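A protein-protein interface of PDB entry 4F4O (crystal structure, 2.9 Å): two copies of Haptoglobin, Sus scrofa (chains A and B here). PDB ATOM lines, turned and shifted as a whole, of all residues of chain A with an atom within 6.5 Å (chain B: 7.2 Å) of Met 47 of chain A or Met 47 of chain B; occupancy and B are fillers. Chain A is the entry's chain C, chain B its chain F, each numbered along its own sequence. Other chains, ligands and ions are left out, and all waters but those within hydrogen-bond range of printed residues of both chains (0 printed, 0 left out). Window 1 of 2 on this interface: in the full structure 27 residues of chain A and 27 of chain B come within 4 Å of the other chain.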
ATOM      1  N   VAL A  44       6.674  24.355 -16.513  1.00  0.00           N
ATOM      2  CA  VAL A  44       7.112  23.007 -16.845  1.00  0.00           C
ATOM      3  C   VAL A  44       8.640  22.860 -16.850  1.00  0.00           C
ATOM      4  O   VAL A  44       9.371  23.755 -17.292  1.00  0.00           O
ATOM      5  CB  VAL A  44       6.517  22.589 -18.192  1.00  0.00           C
ATOM      6  CG1 VAL A  44       7.324  21.511 -18.828  1.00  0.00           C
ATOM      7  CG2 VAL A  44       5.081  22.144 -18.003  1.00  0.00           C
ATOM      8  N   GLU A  45       9.113  21.740 -16.313  1.00  0.00           N
ATOM      9  CA  GLU A  45      10.523  21.399 -16.353  1.00  0.00           C
ATOM     10  C   GLU A  45      10.686  20.243 -17.338  1.00  0.00           C
ATOM     11  O   GLU A  45       9.945  19.262 -17.253  1.00  0.00           O
ATOM     12  CB  GLU A  45      10.961  20.974 -14.960  1.00  0.00           C
ATOM     13  CG  GLU A  45      12.444  21.006 -14.726  1.00  0.00           C
ATOM     14  CD  GLU A  45      12.825  20.446 -13.369  1.00  0.00           C
ATOM     15  OE1 GLU A  45      12.054  19.627 -12.804  1.00  0.00           O
ATOM     16  OE2 GLU A  45      13.905  20.830 -12.871  1.00  0.00           O
ATOM     17  N   HIS A  46      11.622  20.352 -18.280  1.00  0.00           N
ATOM     18  CA  HIS A  46      11.835  19.259 -19.254  1.00  0.00           C
ATOM     19  C   HIS A  46      12.911  18.233 -18.862  1.00  0.00           C
ATOM     20  O   HIS A  46      13.992  18.595 -18.413  1.00  0.00           O
ATOM     21  CB  HIS A  46      12.129  19.806 -20.660  1.00  0.00           C
ATOM     22  CG  HIS A  46      10.924  20.358 -21.365  1.00  0.00           C
ATOM     23  ND1 HIS A  46      10.641  21.708 -21.414  1.00  0.00           N
ATOM     24  CD2 HIS A  46       9.928  19.740 -22.045  1.00  0.00           C
ATOM     25  CE1 HIS A  46       9.525  21.899 -22.098  1.00  0.00           C
ATOM     26  NE2 HIS A  46       9.072  20.722 -22.490  1.00  0.00           N
ATOM     27  N   MET A  47      12.606  16.952 -19.035  1.00  0.00           N
ATOM     28  CA  MET A  47      13.602  15.906 -18.818  1.00  0.00           C
ATOM     29  C   MET A  47      13.636  14.910 -19.979  1.00  0.00           C
ATOM     30  O   MET A  47      12.758  14.895 -20.846  1.00  0.00           O
ATOM     31  CB  MET A  47      13.334  15.148 -17.517  1.00  0.00           C
ATOM     32  CG  MET A  47      13.124  16.029 -16.312  1.00  0.00           C
ATOM     33  SD  MET A  47      11.970  15.270 -15.152  1.00  0.00           S
ATOM     34  CE  MET A  47      13.085  14.439 -14.005  1.00  0.00           C
ATOM     35  N   VAL A  48      14.678  14.089 -20.000  1.00  0.00           N
ATOM     36  CA  VAL A  48      14.736  12.929 -20.892  1.00  0.00           C
ATOM     37  C   VAL A  48      15.350  11.751 -20.162  1.00  0.00           C
ATOM     38  O   VAL A  48      16.198  11.926 -19.290  1.00  0.00           O
ATOM     39  CB  VAL A  48      15.563  13.198 -22.142  1.00  0.00           C
ATOM     40  CG1 VAL A  48      14.737  13.942 -23.161  1.00  0.00           C
ATOM     41  CG2 VAL A  48      16.820  13.977 -21.781  1.00  0.00           C
ATOM     42  N   ARG A  49      14.885  10.554 -20.493  1.00  0.00           N
ATOM     43  CA  ARG A  49      15.556   9.336 -20.065  1.00  0.00           C
ATOM     44  C   ARG A  49      16.077   8.637 -21.319  1.00  0.00           C
ATOM     45  O   ARG A  49      15.336   8.468 -22.284  1.00  0.00           O
ATOM     46  CB  ARG A  49      14.607   8.423 -19.283  1.00  0.00           C
ATOM     47  CG  ARG A  49      15.212   7.056 -18.965  1.00  0.00           C
ATOM     48  CD  ARG A  49      14.317   6.191 -18.078  1.00  0.00           C
ATOM     49  NE  ARG A  49      14.105   6.801 -16.769  1.00  0.00           N
ATOM     50  CZ  ARG A  49      12.928   7.263 -16.332  1.00  0.00           C
ATOM     51  NH1 ARG A  49      11.846   7.156 -17.106  1.00  0.00           N
ATOM     52  NH2 ARG A  49      12.824   7.813 -15.117  1.00  0.00           N
ATOM     53  N   VAL A  65      18.546   9.799 -16.555  1.00  0.00           N
ATOM     54  CA  VAL A  65      17.637  10.934 -16.668  1.00  0.00           C
ATOM     55  C   VAL A  65      18.385  12.269 -16.645  1.00  0.00           C
ATOM     56  O   VAL A  65      19.181  12.550 -15.736  1.00  0.00           O
ATOM     57  CB  VAL A  65      16.524  10.899 -15.598  1.00  0.00           C
ATOM     58  CG1 VAL A  65      15.654  12.151 -15.676  1.00  0.00           C
ATOM     59  CG2 VAL A  65      15.682   9.664 -15.784  1.00  0.00           C
ATOM     60  N   TYR A  66      18.120  13.080 -17.665  1.00  0.00           N
ATOM     61  CA  TYR A  66      18.792  14.357 -17.845  1.00  0.00           C
ATOM     62  C   TYR A  66      17.760  15.438 -17.925  1.00  0.00           C
ATOM     63  O   TYR A  66      16.678  15.231 -18.470  1.00  0.00           O
ATOM     64  CB  TYR A  66      19.656  14.337 -19.105  1.00  0.00           C
ATOM     65  CG  TYR A  66      20.870  13.522 -18.869  1.00  0.00           C
ATOM     66  CD1 TYR A  66      20.811  12.153 -18.944  1.00  0.00           C
ATOM     67  CD2 TYR A  66      22.062  14.113 -18.492  1.00  0.00           C
ATOM     68  CE1 TYR A  66      21.905  11.386 -18.674  1.00  0.00           C
ATOM     69  CE2 TYR A  66      23.180  13.353 -18.240  1.00  0.00           C
ATOM     70  CZ  TYR A  66      23.099  11.982 -18.326  1.00  0.00           C
ATOM     71  OH  TYR A  66      24.206  11.197 -18.061  1.00  0.00           O
ATOM     72  N   THR A  67      18.095  16.603 -17.392  1.00  0.00           N
ATOM     73  CA  THR A  67      17.082  17.606 -17.172  1.00  0.00           C
ATOM     74  C   THR A  67      17.590  19.018 -17.515  1.00  0.00           C
ATOM     75  O   THR A  67      18.710  19.398 -17.149  1.00  0.00           O
ATOM     76  CB  THR A  67      16.499  17.446 -15.738  1.00  0.00           C
ATOM     77  OG1 THR A  67      16.051  18.709 -15.235  1.00  0.00           O
ATOM     78  CG2 THR A  67      17.549  16.845 -14.795  1.00  0.00           C
ATOM     79  N   LEU A  68      16.750  19.771 -18.234  1.00  0.00           N
ATOM     80  CA  LEU A  68      17.083  21.092 -18.792  1.00  0.00           C
ATOM     81  C   LEU A  68      17.282  22.208 -17.767  1.00  0.00           C
ATOM     82  O   LEU A  68      16.390  22.497 -16.994  1.00  0.00           O
ATOM     83  CB  LEU A  68      15.971  21.539 -19.744  1.00  0.00           C
ATOM     84  CG  LEU A  68      16.377  21.944 -21.162  1.00  0.00           C
ATOM     85  CD1 LEU A  68      15.160  22.413 -21.955  1.00  0.00           C
ATOM     86  CD2 LEU A  68      17.461  23.008 -21.141  1.00  0.00           C
ATOM     87  N   TRP A  74      21.581  20.239 -20.518  1.00  0.00           N
ATOM     88  CA  TRP A  74      20.925  19.015 -20.096  1.00  0.00           C
ATOM     89  C   TRP A  74      21.831  18.308 -19.103  1.00  0.00           C
ATOM     90  O   TRP A  74      22.942  17.871 -19.448  1.00  0.00           O
ATOM     91  CB  TRP A  74      20.632  18.136 -21.292  1.00  0.00           C
ATOM     92  CG  TRP A  74      19.608  18.731 -22.165  1.00  0.00           C
ATOM     93  CD1 TRP A  74      19.800  19.667 -23.140  1.00  0.00           C
ATOM     94  CD2 TRP A  74      18.206  18.449 -22.148  1.00  0.00           C
ATOM     95  NE1 TRP A  74      18.599  19.978 -23.740  1.00  0.00           N
ATOM     96  CE2 TRP A  74      17.605  19.239 -23.150  1.00  0.00           C
ATOM     97  CE3 TRP A  74      17.402  17.597 -21.390  1.00  0.00           C
ATOM     98  CZ2 TRP A  74      16.243  19.200 -23.416  1.00  0.00           C
ATOM     99  CZ3 TRP A  74      16.060  17.556 -21.657  1.00  0.00           C
ATOM    100  CH2 TRP A  74      15.490  18.350 -22.663  1.00  0.00           C
ATOM    101  N   PRO B  36      16.923  17.737 -26.744  1.00  0.00           N
ATOM    102  CA  PRO B  36      17.995  17.112 -25.957  1.00  0.00           C
ATOM    103  C   PRO B  36      19.024  16.490 -26.881  1.00  0.00           C
ATOM    104  O   PRO B  36      18.701  16.122 -28.023  1.00  0.00           O
ATOM    105  CB  PRO B  36      17.260  16.032 -25.155  1.00  0.00           C
ATOM    106  CG  PRO B  36      16.136  15.619 -26.056  1.00  0.00           C
ATOM    107  CD  PRO B  36      15.758  16.842 -26.893  1.00  0.00           C
ATOM    108  N   VAL B  44      15.767   8.938 -27.096  1.00  0.00           N
ATOM    109  CA  VAL B  44      15.223   9.575 -25.905  1.00  0.00           C
ATOM    110  C   VAL B  44      13.763   9.223 -25.622  1.00  0.00           C
ATOM    111  O   VAL B  44      12.970   9.004 -26.533  1.00  0.00           O
ATOM    112  CB  VAL B  44      15.392  11.111 -25.933  1.00  0.00           C
ATOM    113  CG1 VAL B  44      16.738  11.501 -25.354  1.00  0.00           C
ATOM    114  CG2 VAL B  44      15.244  11.641 -27.344  1.00  0.00           C
ATOM    115  N   GLU B  45      13.442   9.130 -24.335  1.00  0.00           N
ATOM    116  CA  GLU B  45      12.062   9.090 -23.856  1.00  0.00           C
ATOM    117  C   GLU B  45      11.764  10.415 -23.143  1.00  0.00           C
ATOM    118  O   GLU B  45      12.403  10.729 -22.134  1.00  0.00           O
ATOM    119  CB  GLU B  45      11.874   7.922 -22.888  1.00  0.00           C
ATOM    120  CG  GLU B  45      10.610   7.996 -22.057  1.00  0.00           C
ATOM    121  CD  GLU B  45      10.431   6.792 -21.153  1.00  0.00           C
ATOM    122  OE1 GLU B  45      11.431   6.291 -20.591  1.00  0.00           O
ATOM    123  OE2 GLU B  45       9.278   6.343 -21.009  1.00  0.00           O
ATOM    124  N   HIS B  46      10.820  11.200 -23.667  1.00  0.00           N
ATOM    125  CA  HIS B  46      10.542  12.530 -23.111  1.00  0.00           C
ATOM    126  C   HIS B  46       9.686  12.535 -21.852  1.00  0.00           C
ATOM    127  O   HIS B  46       8.708  11.799 -21.737  1.00  0.00           O
ATOM    128  CB  HIS B  46       9.884  13.429 -24.151  1.00  0.00           C
ATOM    129  CG  HIS B  46      10.842  13.991 -25.148  1.00  0.00           C
ATOM    130  ND1 HIS B  46      11.077  13.397 -26.368  1.00  0.00           N
ATOM    131  CD2 HIS B  46      11.632  15.093 -25.103  1.00  0.00           C
ATOM    132  CE1 HIS B  46      11.970  14.108 -27.036  1.00  0.00           C
ATOM    133  NE2 HIS B  46      12.321  15.142 -26.291  1.00  0.00           N
ATOM    134  N   MET B  47      10.064  13.387 -20.909  1.00  0.00           N
ATOM    135  CA  MET B  47       9.281  13.598 -19.695  1.00  0.00           C
ATOM    136  C   MET B  47       9.163  15.080 -19.380  1.00  0.00           C
ATOM    137  O   MET B  47       9.926  15.901 -19.887  1.00  0.00           O
ATOM    138  CB  MET B  47       9.931  12.892 -18.508  1.00  0.00           C
ATOM    139  CG  MET B  47      10.490  11.523 -18.834  1.00  0.00           C
ATOM    140  SD  MET B  47      11.335  10.822 -17.415  1.00  0.00           S
ATOM    141  CE  MET B  47      10.055   9.730 -16.770  1.00  0.00           C
ATOM    142  N   VAL B  48       8.188  15.416 -18.546  1.00  0.00           N
ATOM    143  CA  VAL B  48       8.092  16.751 -17.937  1.00  0.00           C
ATOM    144  C   VAL B  48       7.702  16.617 -16.473  1.00  0.00           C
ATOM    145  O   VAL B  48       6.943  15.706 -16.123  1.00  0.00           O
ATOM    146  CB  VAL B  48       7.071  17.677 -18.644  1.00  0.00           C
ATOM    147  CG1 VAL B  48       7.599  18.137 -19.995  1.00  0.00           C
ATOM    148  CG2 VAL B  48       5.718  16.987 -18.786  1.00  0.00           C
ATOM    149  N   ARG B  49       8.256  17.488 -15.623  1.00  0.00           N
ATOM    150  CA  ARG B  49       7.777  17.654 -14.249  1.00  0.00           C
ATOM    151  C   ARG B  49       7.074  18.993 -14.131  1.00  0.00           C
ATOM    152  O   ARG B  49       7.647  20.028 -14.463  1.00  0.00           O
ATOM    153  CB  ARG B  49       8.921  17.598 -13.233  1.00  0.00           C
ATOM    154  CG  ARG B  49       8.474  17.906 -11.817  1.00  0.00           C
ATOM    155  CD  ARG B  49       9.558  17.688 -10.784  1.00  0.00           C
ATOM    156  NE  ARG B  49       9.939  16.286 -10.700  1.00  0.00           N
ATOM    157  CZ  ARG B  49      11.091  15.801 -11.178  1.00  0.00           C
ATOM    158  NH1 ARG B  49      11.968  16.627 -11.754  1.00  0.00           N
ATOM    159  NH2 ARG B  49      11.381  14.495 -11.088  1.00  0.00           N
ATOM    160  N   VAL B  65       5.061  14.144 -12.648  1.00  0.00           N
ATOM    161  CA  VAL B  65       5.866  13.812 -13.807  1.00  0.00           C
ATOM    162  C   VAL B  65       5.094  12.975 -14.862  1.00  0.00           C
ATOM    163  O   VAL B  65       4.540  11.931 -14.552  1.00  0.00           O
ATOM    164  CB  VAL B  65       7.123  13.068 -13.353  1.00  0.00           C
ATOM    165  CG1 VAL B  65       7.837  12.588 -14.572  1.00  0.00           C
ATOM    166  CG2 VAL B  65       7.994  13.982 -12.534  1.00  0.00           C
ATOM    167  N   TYR B  66       5.068  13.529 -16.083  1.00  0.00           N
ATOM    168  CA  TYR B  66       4.338  12.968 -17.197  1.00  0.00           C
ATOM    169  C   TYR B  66       5.325  12.616 -18.287  1.00  0.00           C
ATOM    170  O   TYR B  66       6.133  13.452 -18.710  1.00  0.00           O
ATOM    171  CB  TYR B  66       3.298  13.961 -17.709  1.00  0.00           C
ATOM    172  CG  TYR B  66       2.219  14.258 -16.691  1.00  0.00           C
ATOM    173  CD1 TYR B  66       2.475  15.080 -15.590  1.00  0.00           C
ATOM    174  CD2 TYR B  66       0.953  13.720 -16.825  1.00  0.00           C
ATOM    175  CE1 TYR B  66       1.503  15.351 -14.646  1.00  0.00           C
ATOM    176  CE2 TYR B  66      -0.031  13.991 -15.893  1.00  0.00           C
ATOM    177  CZ  TYR B  66       0.244  14.810 -14.800  1.00  0.00           C
ATOM    178  OH  TYR B  66      -0.744  15.072 -13.866  1.00  0.00           O
ATOM    179  N   THR B  67       5.273  11.363 -18.722  1.00  0.00           N
ATOM    180  CA  THR B  67       6.144  10.900 -19.784  1.00  0.00           C
ATOM    181  C   THR B  67       5.318  10.730 -21.068  1.00  0.00           C
ATOM    182  O   THR B  67       4.118  10.447 -21.021  1.00  0.00           O
ATOM    183  CB  THR B  67       6.896   9.608 -19.362  1.00  0.00           C
ATOM    184  OG1 THR B  67       6.499   8.514 -20.196  1.00  0.00           O
ATOM    185  CG2 THR B  67       6.614   9.255 -17.892  1.00  0.00           C
ATOM    186  N   LEU B  68       5.957  10.948 -22.210  1.00  0.00           N
ATOM    187  CA  LEU B  68       5.266  10.901 -23.501  1.00  0.00           C
ATOM    188  C   LEU B  68       4.983   9.477 -24.018  1.00  0.00           C
ATOM    189  O   LEU B  68       5.891   8.651 -24.139  1.00  0.00           O
ATOM    190  CB  LEU B  68       6.058  11.703 -24.534  1.00  0.00           C
ATOM    191  CG  LEU B  68       5.411  12.114 -25.852  1.00  0.00           C
ATOM    192  CD1 LEU B  68       4.021  12.661 -25.645  1.00  0.00           C
ATOM    193  CD2 LEU B  68       6.282  13.176 -26.434  1.00  0.00           C
ATOM    194  N   TRP B  74       0.745  12.766 -23.093  1.00  0.00           N
ATOM    195  CA  TRP B  74       1.468  12.858 -21.834  1.00  0.00           C
ATOM    196  C   TRP B  74       0.763  12.126 -20.716  1.00  0.00           C
ATOM    197  O   TRP B  74      -0.392  12.398 -20.431  1.00  0.00           O
ATOM    198  CB  TRP B  74       1.641  14.306 -21.459  1.00  0.00           C
ATOM    199  CG  TRP B  74       2.487  15.002 -22.429  1.00  0.00           C
ATOM    200  CD1 TRP B  74       2.078  15.670 -23.544  1.00  0.00           C
ATOM    201  CD2 TRP B  74       3.917  15.094 -22.401  1.00  0.00           C
ATOM    202  NE1 TRP B  74       3.168  16.192 -24.205  1.00  0.00           N
ATOM    203  CE2 TRP B  74       4.307  15.851 -23.523  1.00  0.00           C
ATOM    204  CE3 TRP B  74       4.902  14.618 -21.530  1.00  0.00           C
ATOM    205  CZ2 TRP B  74       5.648  16.144 -23.794  1.00  0.00           C
ATOM    206  CZ3 TRP B  74       6.227  14.907 -21.802  1.00  0.00           C
ATOM    207  CH2 TRP B  74       6.587  15.665 -22.921  1.00  0.00           C
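The side-chain carboxylate (OE1) of Glu 45 of chain A lies within salt-bridge range of the guanidinium group (NH1) of Arg 49 of chain B (3.2 Å). O of Met 47 of chain B is in hydrogen-bond range of N of Met 47 of chain A, 3.0 Å away. SD of Met 47 of chain A lies close to NH1 of Arg 49 of chain B (3.7 Å). OE1 of Glu 45 of chain B is in salt-bridge range of NH1 of Arg 49 of chain A. NH1 of Arg 49 of chain A lies close to SD of Met 47 of chain B.
N of Leu 68 of chain A sits at hydrogen-bond distance from O of His 46 of chain A, 3.0 Å away. The backbone NH (N) of Val 48 of chain A sits at hydrogen-bond distance from the backbone carbonyl oxygen (O) of Tyr 66 of chain A (2.8 Å). The backbone NH of Leu 68 of chain B is in hydrogen-bond range of the backbone carbonyl oxygen of His 46 of chain B (2.9 Å). O of Tyr 66 of chain B sits at hydrogen-bond distance from N of Val 48 of chain B.
Val 44 of chain A touches Val 48 of chain B (CG1 to CG1, 3.6 Å). Arg 49 of chain B touches Val 44 of chain A (O to C, 3.8 Å). Val 48 of chain B touches Glu 45 of chain A (CA to O, 3.2 Å). His 46 of chain A touches Met 47 of chain B. Val 48 of chain B touches His 46 of chain A. CA of His 46 of chain B touches O of Met 47 of chain A, 3.95 Å away. Pro 36 of chain B touches Val 48 of chain A (CG to CG1, 3.6 Å). Glu 45 of chain B touches Val 48 of chain A. O of Arg 49 of chain A touches C of Val 44 of chain B, 3.8 Å away. Trp 74 of chain A touches Pro 36 of chain B.
Of the printed residues of chain B, Glu 45 of chain A touches Val 48 (3.2 Å) and Arg 49 (2.9 Å). Of chain B, only His 46, Met 47 and Arg 49 come within 4 Å of Met 47 of chain A. Of the printed residues of chain B, Val 48 of chain A touches Pro 36, Val 44, Glu 45 and His 46. Printed residues of chain B within 4 Å of Arg 49 of chain A: Val 44 (3.8 Å), Glu 45 (2.9 Å) and Met 47 (3.2 Å). Of chain A, only His 46, Met 47 and Arg 49 come within 4 Å of Met 47 of chain B. The nearest residue of chain B that does not touch Met 47 of chain A is Glu 45 of chain B (4.4 Å). The nearest residue of chain A that does not touch Met 47 of chain B is Glu 45 of chain A (4.3 Å). The nearest printed residue of chain A that does not touch Val 48 of chain B is Met 47 of chain A (4.6 Å).
Of the 11 printed residues of chain A, 7 touch a printed residue of chain B. Hydrophobic or aromatic side chains of chain A that line the printed part of chain B: Val 44, His 46, Met 47, Val 48 and Trp 74. Along chain A the printed residues that touch a printed residue of chain B span positions 44 to 74. Printed residues of chain B that touch a printed residue of chain A: Pro 36, Val 44, Glu 45, His 46, Met 47, Val 48 and Arg 49. Hydrophobic or aromatic side chains of chain B that line the printed part of chain A: Pro 36, Val 44, His 46, Met 47 and Val 48. Along chain B the printed residues that touch a printed residue of chain A span positions 36 to 49.
Val 44 of chain A touches Arg 49 of chain B, and with the chains exchanged Arg 49 of chain A touches Val 44 of chain B. His 46 of chain A touches Met 47 of chain B, and with the chains exchanged Met 47 of chain A touches His 46 of chain B. His 46 of chain A touches Val 48 of chain B, and with the chains exchanged Val 48 of chain A touches His 46 of chain B. Met 47 of chain A touches Arg 49 of chain B, and with the chains exchanged Arg 49 of chain A touches Met 47 of chain B. 11 positions are printed for both chains.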
